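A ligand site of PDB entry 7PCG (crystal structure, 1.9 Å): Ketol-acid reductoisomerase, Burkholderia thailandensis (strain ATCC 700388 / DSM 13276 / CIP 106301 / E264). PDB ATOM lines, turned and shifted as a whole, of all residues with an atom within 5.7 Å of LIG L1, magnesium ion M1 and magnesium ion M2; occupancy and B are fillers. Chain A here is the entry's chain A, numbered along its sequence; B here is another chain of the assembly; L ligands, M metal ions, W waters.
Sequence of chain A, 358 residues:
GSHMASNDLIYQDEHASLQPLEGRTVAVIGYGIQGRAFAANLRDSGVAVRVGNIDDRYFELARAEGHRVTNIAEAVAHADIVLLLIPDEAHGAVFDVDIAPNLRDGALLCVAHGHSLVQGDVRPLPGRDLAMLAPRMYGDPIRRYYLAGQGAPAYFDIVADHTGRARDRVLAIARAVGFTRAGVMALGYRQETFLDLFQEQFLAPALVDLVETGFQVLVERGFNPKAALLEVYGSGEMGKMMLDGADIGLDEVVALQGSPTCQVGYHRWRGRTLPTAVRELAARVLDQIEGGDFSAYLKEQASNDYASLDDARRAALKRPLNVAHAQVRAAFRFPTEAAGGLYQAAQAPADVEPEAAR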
ATOM      1  N   GLU A 231     -17.903  -8.140  27.529  1.00  0.00           N
ATOM      2  CA  GLU A 231     -16.698  -7.886  26.690  1.00  0.00           C
ATOM      3  C   GLU A 231     -17.065  -7.946  25.202  1.00  0.00           C
ATOM      4  O   GLU A 231     -16.634  -7.044  24.465  1.00  0.00           O
ATOM      5  CB  GLU A 231     -15.583  -8.882  27.041  1.00  0.00           C
ATOM      6  CG  GLU A 231     -14.962  -8.635  28.403  1.00  0.00           C
ATOM      7  CD  GLU A 231     -14.743  -7.170  28.738  1.00  0.00           C
ATOM      8  OE1 GLU A 231     -13.877  -6.537  28.101  1.00  0.00           O
ATOM      9  OE2 GLU A 231     -15.448  -6.654  29.632  1.00  0.00           O
ATOM     10  N   GLU A 237     -18.795  -1.309  24.561  1.00  0.00           N
ATOM     11  CA  GLU A 237     -17.426  -0.909  24.102  1.00  0.00           C
ATOM     12  C   GLU A 237     -17.273  -1.216  22.614  1.00  0.00           C
ATOM     13  O   GLU A 237     -16.781  -0.335  21.876  1.00  0.00           O
ATOM     14  CB  GLU A 237     -16.332  -1.602  24.919  1.00  0.00           C
ATOM     15  CG  GLU A 237     -14.977  -0.947  24.733  1.00  0.00           C
ATOM     16  CD  GLU A 237     -13.853  -1.486  25.599  1.00  0.00           C
ATOM     17  OE1 GLU A 237     -13.883  -2.693  25.930  1.00  0.00           O
ATOM     18  OE2 GLU A 237     -12.947  -0.698  25.940  1.00  0.00           O
ATOM     19  N   GLN A 257      -7.716   5.530  20.921  1.00  0.00           N
ATOM     20  CA  GLN A 257      -8.407   5.157  22.182  1.00  0.00           C
ATOM     21  C   GLN A 257      -7.789   3.908  22.814  1.00  0.00           C
ATOM     22  O   GLN A 257      -8.126   3.630  23.984  1.00  0.00           O
ATOM     23  CB  GLN A 257      -9.902   4.913  21.928  1.00  0.00           C
ATOM     24  CG  GLN A 257     -10.622   6.082  21.277  1.00  0.00           C
ATOM     25  CD  GLN A 257     -10.731   7.287  22.176  1.00  0.00           C
ATOM     26  OE1 GLN A 257      -9.986   7.443  23.140  1.00  0.00           O
ATOM     27  NE2 GLN A 257     -11.672   8.161  21.858  1.00  0.00           N
ATOM     28  N   GLY A 258      -6.950   3.174  22.077  1.00  0.00           N
ATOM     29  CA  GLY A 258      -6.361   1.903  22.531  1.00  0.00           C
ATOM     30  C   GLY A 258      -5.072   2.120  23.312  1.00  0.00           C
ATOM     31  O   GLY A 258      -4.241   2.936  22.880  1.00  0.00           O
ATOM     32  N   SER A 259      -4.913   1.424  24.448  1.00  0.00           N
ATOM     33  CA  SER A 259      -3.623   1.270  25.166  1.00  0.00           C
ATOM     34  C   SER A 259      -2.599   0.666  24.213  1.00  0.00           C
ATOM     35  O   SER A 259      -2.993   0.001  23.258  1.00  0.00           O
ATOM     36  CB  SER A 259      -3.790   0.416  26.402  1.00  0.00           C
ATOM     37  OG  SER A 259      -4.025  -0.938  26.044  1.00  0.00           O
ATOM     38  N   THR A 261      -0.766  -1.930  24.681  1.00  0.00           N
ATOM     39  CA  THR A 261      -1.040  -3.393  24.793  1.00  0.00           C
ATOM     40  C   THR A 261      -2.161  -3.764  23.807  1.00  0.00           C
ATOM     41  O   THR A 261      -1.977  -4.754  23.067  1.00  0.00           O
ATOM     42  CB  THR A 261      -1.395  -3.794  26.230  1.00  0.00           C
ATOM     43  OG1 THR A 261      -0.249  -3.550  27.056  1.00  0.00           O
ATOM     44  CG2 THR A 261      -1.810  -5.243  26.366  1.00  0.00           C
ATOM     45  N   CYS A 262      -3.255  -2.998  23.810  1.00  0.00           N
ATOM     46  CA  CYS A 262      -4.442  -3.190  22.937  1.00  0.00           C
ATOM     47  C   CYS A 262      -4.028  -3.101  21.462  1.00  0.00           C
ATOM     48  O   CYS A 262      -4.400  -4.008  20.689  1.00  0.00           O
ATOM     49  CB  CYS A 262      -5.526  -2.166  23.251  1.00  0.00           C
ATOM     50  SG  CYS A 262      -6.879  -2.138  22.044  1.00  0.00           S
ATOM     51  N   HIS B 113      -5.872  -2.871  34.840  1.00  0.00           N
ATOM     52  CA  HIS B 113      -5.667  -4.088  33.999  1.00  0.00           C
ATOM     53  C   HIS B 113      -4.757  -5.046  34.768  1.00  0.00           C
ATOM     54  O   HIS B 113      -3.779  -4.561  35.387  1.00  0.00           O
ATOM     55  CB  HIS B 113      -5.123  -3.666  32.632  1.00  0.00           C
ATOM     56  CG  HIS B 113      -4.930  -4.776  31.653  1.00  0.00           C
ATOM     57  ND1 HIS B 113      -5.864  -5.782  31.474  1.00  0.00           N
ATOM     58  CD2 HIS B 113      -3.939  -5.009  30.760  1.00  0.00           C
ATOM     59  CE1 HIS B 113      -5.431  -6.613  30.539  1.00  0.00           C
ATOM     60  NE2 HIS B 113      -4.262  -6.163  30.077  1.00  0.00           N
ATOM     61  N   PRO B 135     -12.031  -0.628  34.165  1.00  0.00           N
ATOM     62  CA  PRO B 135     -13.228  -0.233  33.416  1.00  0.00           C
ATOM     63  C   PRO B 135     -13.353  -1.057  32.131  1.00  0.00           C
ATOM     64  O   PRO B 135     -12.325  -1.449  31.582  1.00  0.00           O
ATOM     65  CB  PRO B 135     -13.030   1.251  33.095  1.00  0.00           C
ATOM     66  CG  PRO B 135     -11.858   1.698  33.962  1.00  0.00           C
ATOM     67  CD  PRO B 135     -11.041   0.452  34.238  1.00  0.00           C
ATOM     68  N   ARG B 136     -14.591  -1.299  31.672  1.00  0.00           N
ATOM     69  CA  ARG B 136     -14.890  -2.093  30.447  1.00  0.00           C
ATOM     70  C   ARG B 136     -15.172  -1.131  29.291  1.00  0.00           C
ATOM     71  O   ARG B 136     -15.951  -1.496  28.392  1.00  0.00           O
ATOM     72  CB  ARG B 136     -16.094  -3.018  30.687  1.00  0.00           C
ATOM     73  CG  ARG B 136     -16.054  -3.807  31.991  1.00  0.00           C
ATOM     74  CD  ARG B 136     -14.669  -4.274  32.407  1.00  0.00           C
ATOM     75  NE  ARG B 136     -13.967  -5.057  31.403  1.00  0.00           N
ATOM     76  CZ  ARG B 136     -12.668  -5.354  31.436  1.00  0.00           C
ATOM     77  NH1 ARG B 136     -11.902  -4.905  32.422  1.00  0.00           N
ATOM     78  NH2 ARG B 136     -12.132  -6.082  30.472  1.00  0.00           N
ATOM     79  N   MET B 137     -14.527   0.038  29.299  1.00  0.00           N
ATOM     80  CA  MET B 137     -14.813   1.170  28.379  1.00  0.00           C
ATOM     81  C   MET B 137     -13.581   2.090  28.325  1.00  0.00           C
ATOM     82  O   MET B 137     -12.852   2.139  29.327  1.00  0.00           O
ATOM     83  CB  MET B 137     -16.029   1.968  28.882  1.00  0.00           C
ATOM     84  CG  MET B 137     -16.492   3.062  27.963  1.00  0.00           C
ATOM     85  SD  MET B 137     -16.970   2.487  26.321  1.00  0.00           S
ATOM     86  CE  MET B 137     -18.434   1.537  26.713  1.00  0.00           C
ATOM     87  N   TYR B 138     -13.381   2.785  27.202  1.00  0.00           N
ATOM     88  CA  TYR B 138     -12.268   3.759  27.031  1.00  0.00           C
ATOM     89  C   TYR B 138     -12.711   5.129  27.565  1.00  0.00           C
ATOM     90  O   TYR B 138     -13.854   5.259  28.022  1.00  0.00           O
ATOM     91  CB  TYR B 138     -11.736   3.758  25.599  1.00  0.00           C
ATOM     92  CG  TYR B 138     -12.730   3.875  24.465  1.00  0.00           C
ATOM     93  CD1 TYR B 138     -13.306   2.748  23.905  1.00  0.00           C
ATOM     94  CD2 TYR B 138     -13.021   5.100  23.893  1.00  0.00           C
ATOM     95  CE1 TYR B 138     -14.195   2.841  22.838  1.00  0.00           C
ATOM     96  CE2 TYR B 138     -13.898   5.213  22.819  1.00  0.00           C
ATOM     97  CZ  TYR B 138     -14.482   4.089  22.296  1.00  0.00           C
ATOM     98  OH  TYR B 138     -15.348   4.195  21.247  1.00  0.00           O
ATOM     99  N   GLU B 192      -9.477 -11.314  34.205  1.00  0.00           N
ATOM    100  CA  GLU B 192      -9.668  -9.978  33.584  1.00  0.00           C
ATOM    101  C   GLU B 192      -8.624  -9.785  32.485  1.00  0.00           C
ATOM    102  O   GLU B 192      -9.008  -9.361  31.380  1.00  0.00           O
ATOM    103  CB  GLU B 192      -9.550  -8.850  34.619  1.00  0.00           C
ATOM    104  CG  GLU B 192      -9.956  -7.481  34.092  1.00  0.00           C
ATOM    105  CD  GLU B 192      -8.929  -6.731  33.245  1.00  0.00           C
ATOM    106  OE1 GLU B 192      -7.718  -6.985  33.409  1.00  0.00           O
ATOM    107  OE2 GLU B 192      -9.353  -5.884  32.435  1.00  0.00           O
ATOM    108  N   ASP B 196      -9.694  -9.452  28.608  1.00  0.00           N
ATOM    109  CA  ASP B 196      -9.387  -8.112  28.038  1.00  0.00           C
ATOM    110  C   ASP B 196      -8.573  -8.291  26.751  1.00  0.00           C
ATOM    111  O   ASP B 196      -8.951  -7.680  25.732  1.00  0.00           O
ATOM    112  CB  ASP B 196      -8.652  -7.247  29.066  1.00  0.00           C
ATOM    113  CG  ASP B 196      -8.711  -5.769  28.757  1.00  0.00           C
ATOM    114  OD1 ASP B 196      -9.813  -5.191  28.851  1.00  0.00           O
ATOM    115  OD2 ASP B 196      -7.661  -5.203  28.396  1.00  0.00           O
ATOM    116  N   LEU B 197      -7.519  -9.108  26.799  1.00  0.00           N
ATOM    117  CA  LEU B 197      -6.609  -9.349  25.652  1.00  0.00           C
ATOM    118  C   LEU B 197      -7.351 -10.106  24.540  1.00  0.00           C
ATOM    119  O   LEU B 197      -7.044  -9.851  23.368  1.00  0.00           O
ATOM    120  CB  LEU B 197      -5.369 -10.116  26.128  1.00  0.00           C
ATOM    121  CG  LEU B 197      -4.472  -9.383  27.127  1.00  0.00           C
ATOM    122  CD1 LEU B 197      -3.217 -10.197  27.440  1.00  0.00           C
ATOM    123  CD2 LEU B 197      -4.085  -8.000  26.632  1.00  0.00           C
ATOM    124  N   GLN B 199     -10.661  -9.885  23.774  1.00  0.00           N
ATOM    125  CA  GLN B 199     -11.516  -8.864  23.120  1.00  0.00           C
ATOM    126  C   GLN B 199     -10.676  -8.057  22.116  1.00  0.00           C
ATOM    127  O   GLN B 199     -11.194  -7.749  21.017  1.00  0.00           O
ATOM    128  CB  GLN B 199     -12.125  -7.931  24.161  1.00  0.00           C
ATOM    129  CG  GLN B 199     -13.234  -7.042  23.616  1.00  0.00           C
ATOM    130  CD  GLN B 199     -13.261  -5.677  24.249  1.00  0.00           C
ATOM    131  OE1 GLN B 199     -12.264  -4.959  24.267  1.00  0.00           O
ATOM    132  NE2 GLN B 199     -14.414  -5.291  24.778  1.00  0.00           N
ATOM    133  N   GLU B 200      -9.427  -7.748  22.470  1.00  0.00           N
ATOM    134  CA  GLU B 200      -8.518  -6.872  21.680  1.00  0.00           C
ATOM    135  C   GLU B 200      -7.846  -7.650  20.539  1.00  0.00           C
ATOM    136  O   GLU B 200      -7.504  -6.995  19.527  1.00  0.00           O
ATOM    137  CB  GLU B 200      -7.472  -6.255  22.604  1.00  0.00           C
ATOM    138  CG  GLU B 200      -8.074  -5.298  23.625  1.00  0.00           C
ATOM    139  CD  GLU B 200      -7.179  -4.933  24.801  1.00  0.00           C
ATOM    140  OE1 GLU B 200      -6.046  -5.471  24.874  1.00  0.00           O
ATOM    141  OE2 GLU B 200      -7.610  -4.120  25.651  1.00  0.00           O
HETATM  142  C1  LIG L   1      -7.474  -0.797  25.952  1.00  0.00           C
HETATM  143  C2  LIG L   1      -9.019  -0.933  25.974  1.00  0.00           C
HETATM  144  C3  LIG L   1      -9.637  -1.724  27.160  1.00  0.00           C
HETATM  145  C4  LIG L   1      -9.786   0.146  25.396  1.00  0.00           C
HETATM  146  C5  LIG L   1      -9.655  -1.084  24.719  1.00  0.00           C
HETATM  147  O1  LIG L   1      -6.775  -1.468  26.753  1.00  0.00           O
HETATM  148  O2  LIG L   1     -10.877  -1.631  27.336  1.00  0.00           O
HETATM  149  O3  LIG L   1      -8.880  -2.430  27.862  1.00  0.00           O
HETATM  150  O4  LIG L   1      -7.010  -0.033  25.087  1.00  0.00           O
HETATM  151  P1  LG2 L   2      -2.055   5.676  27.161  1.00  0.00           P
HETATM  152  O1  LG2 L   2      -1.311   5.159  25.980  1.00  0.00           O
HETATM  153  O2  LG2 L   2      -3.121   6.696  26.949  1.00  0.00           O
HETATM  154  O3  LG2 L   2      -1.004   6.202  28.256  1.00  0.00           O
HETATM  155  C1  LG2 L   2      -0.468   7.526  28.141  1.00  0.00           C
HETATM  156  C2  LG2 L   2       0.050   7.946  29.496  1.00  0.00           C
HETATM  157  O4  LG2 L   2       1.123   7.053  29.895  1.00  0.00           O
HETATM  158  C3  LG2 L   2       0.640   9.364  29.554  1.00  0.00           C
HETATM  159  O5  LG2 L   2       0.316   9.989  30.795  1.00  0.00           O
HETATM  160  C4  LG2 L   2       2.131   9.099  29.386  1.00  0.00           C
HETATM  161  O6  LG2 L   2       2.948  10.116  29.914  1.00  0.00           O
HETATM  162  C5  LG2 L   2       2.274   7.808  30.193  1.00  0.00           C
HETATM  163  N1  LG2 L   2       3.457   7.027  29.877  1.00  0.00           N
HETATM  164  C6  LG2 L   2       3.757   6.421  28.675  1.00  0.00           C
HETATM  165  N2  LG2 L   2       4.893   5.784  28.685  1.00  0.00           N
HETATM  166  C7  LG2 L   2       5.381   5.965  29.973  1.00  0.00           C
HETATM  167  C8  LG2 L   2       6.561   5.531  30.615  1.00  0.00           C
HETATM  168  N3  LG2 L   2       7.498   4.794  30.018  1.00  0.00           N
HETATM  169  N4  LG2 L   2       6.737   5.892  31.899  1.00  0.00           N
HETATM  170  C9  LG2 L   2       5.796   6.639  32.500  1.00  0.00           C
HETATM  171  N5  LG2 L   2       4.652   7.104  31.996  1.00  0.00           N
HETATM  172  C10 LG2 L   2       4.501   6.729  30.713  1.00  0.00           C
HETATM  173  O7  LG2 L   2      -2.647   4.416  27.965  1.00  0.00           O
HETATM  174  P2  LG2 L   2      -4.074   4.028  28.572  1.00  0.00           P
HETATM  175  O8  LG2 L   2      -4.917   3.504  27.453  1.00  0.00           O
HETATM  176  O9  LG2 L   2      -4.586   5.191  29.360  1.00  0.00           O
HETATM  177  O10 LG2 L   2      -3.680   2.804  29.530  1.00  0.00           O
HETATM  178  C11 LG2 L   2      -3.280   3.011  30.912  1.00  0.00           C
HETATM  179  C12 LG2 L   2      -3.637   1.775  31.718  1.00  0.00           C
HETATM  180  O11 LG2 L   2      -5.068   1.621  31.702  1.00  0.00           O
HETATM  181  C13 LG2 L   2      -3.057   0.445  31.217  1.00  0.00           C
HETATM  182  O12 LG2 L   2      -2.750  -0.409  32.315  1.00  0.00           O
HETATM  183  C14 LG2 L   2      -4.208  -0.117  30.386  1.00  0.00           C
HETATM  184  O13 LG2 L   2      -4.167  -1.528  30.236  1.00  0.00           O
HETATM  185  C15 LG2 L   2      -5.405   0.319  31.220  1.00  0.00           C
HETATM  186  N6  LG2 L   2      -6.681   0.407  30.452  1.00  0.00           N
HETATM  187  C16 LG2 L   2      -6.809   1.231  29.349  1.00  0.00           C
HETATM  188  C17 LG2 L   2      -8.040   1.379  28.716  1.00  0.00           C
HETATM  189  C18 LG2 L   2      -8.197   2.271  27.517  1.00  0.00           C
HETATM  190  O14 LG2 L   2      -9.268   2.847  27.318  1.00  0.00           O
HETATM  191  N7  LG2 L   2      -7.156   2.412  26.699  1.00  0.00           N
HETATM  192  C19 LG2 L   2      -9.144   0.677  29.219  1.00  0.00           C
HETATM  193  C20 LG2 L   2      -9.013  -0.065  30.377  1.00  0.00           C
HETATM  194  C21 LG2 L   2      -7.752  -0.330  30.859  1.00  0.00           C
HETATM  195 MG    MG M   1     -10.909  -3.801  28.131  1.00  0.00          MG
HETATM  196 MG    MG M   2      -6.943  -3.429  27.612  1.00  0.00          MG
HETATM  197  O   HOH W   1     -10.353  -4.433  25.958  1.00  0.00           O
HETATM  198  O   HOH W   2      -6.518  -2.896  29.495  1.00  0.00           O
HETATM  199  O   HOH W   3     -12.881  -4.006  28.053  1.00  0.00           O
HETATM  200  O   HOH W   4      -5.129  -4.299  27.255  1.00  0.00           O
HETATM  201  O   HOH W   5     -10.816  -2.950  30.027  1.00  0.00           O
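O4 of LIG L1 is in hydrogen-bond range of N of Ser 259, 2.6 Å away.
OG of Ser 259 sits at hydrogen-bond distance from O4 of LIG L1 (3.3 Å).
The side-chain carboxylate (OE2) of Glu 237 lies close to an oxygen (O2) of LIG L1 (2.7 Å).
The side-chain sulfur (SG) of Cys 262 sits close to an oxygen (O4) of LIG L1, 3.7 Å away.
O of Gln 257 is in hydrogen-bond range of N7 of LG2 L2 (3.1 Å).
O4 of LIG L1 is in hydrogen-bond range of N7 of LG2 L2 (2.9 Å).
OD1 of Asp 196 of chain B sits close to NH2 of Arg 136 of chain B (3.0 Å).
The backbone NH (N) of Cys 262 is in hydrogen-bond range of the side-chain hydroxyl (OG) of Ser 259, 3.1 Å away.
The side-chain carboxylate of Glu 237 lies within hydrogen-bond range of the side-chain amide nitrogen of Gln 199 of chain B, at 2.9 Å.
The guanidinium group (NE) of Arg 136 of chain B lies within salt-bridge range of the side-chain carboxylate (OE2) of Glu 231 (2.8 Å).
OE2 of Glu 192 of chain B lies within salt-bridge range of NH1 of Arg 136 of chain B (2.7 Å).
Residues that only touch LIG L1: Gly 258 and Gln 257.
Seven residues have an atom within 4 Å of LIG L1: Glu 237, Gln 257, Gly 258, Ser 259, Cys 262, Asp 196 of chain B and Glu 200 of chain B.
The nearest printed residue that does not touch LIG L1 is Tyr 138 of chain B (4.1 Å).
Glu 237 touches magnesium ion M1.
Arg 136 of chain B touches magnesium ion M1.
Three residues have an atom within 4 Å of magnesium ion M1: Glu 237, Arg 136 of chain B and Asp 196 of chain B.
Within 4 Å of magnesium ion M2: Asp 196 of chain B and Glu 200 of chain B.
Magnesium ion M1 is bound by the side-chain carboxylate of Asp 196 of chain B, water W3, water W5, an oxygen (O2) of LIG L1, water W1 and an oxygen (O3) of LIG L1.
Magnesium ion M1 has six donor atoms within binding distance.
Magnesium ion M2 is bound by water W2 (2.0 Å), water W4 (2.0 Å), OD2 of Asp 196 of chain B (2.1 Å), O1 of LIG L1 (2.1 Å), OE2 of Glu 200 of chain B (2.2 Å) and O3 of LIG L1 (2.2 Å).
Magnesium ion M2 has six donor atoms within binding distance.
Water W5 bridges O of Pro 135 of chain B (2.6 Å) and NH1 of Arg 136 of chain B (3.3 Å).
Water W3 lies within hydrogen-bond range of OE1 of Glu 237 (2.7 Å), OE1 of Glu 231 (2.7 Å) and NH2 of Arg 136 of chain B (3.3 Å).
Water W4 bridges the side-chain carboxylate of Glu 200 of chain B and a ring nitrogen (NE2) of His 113 of chain B.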
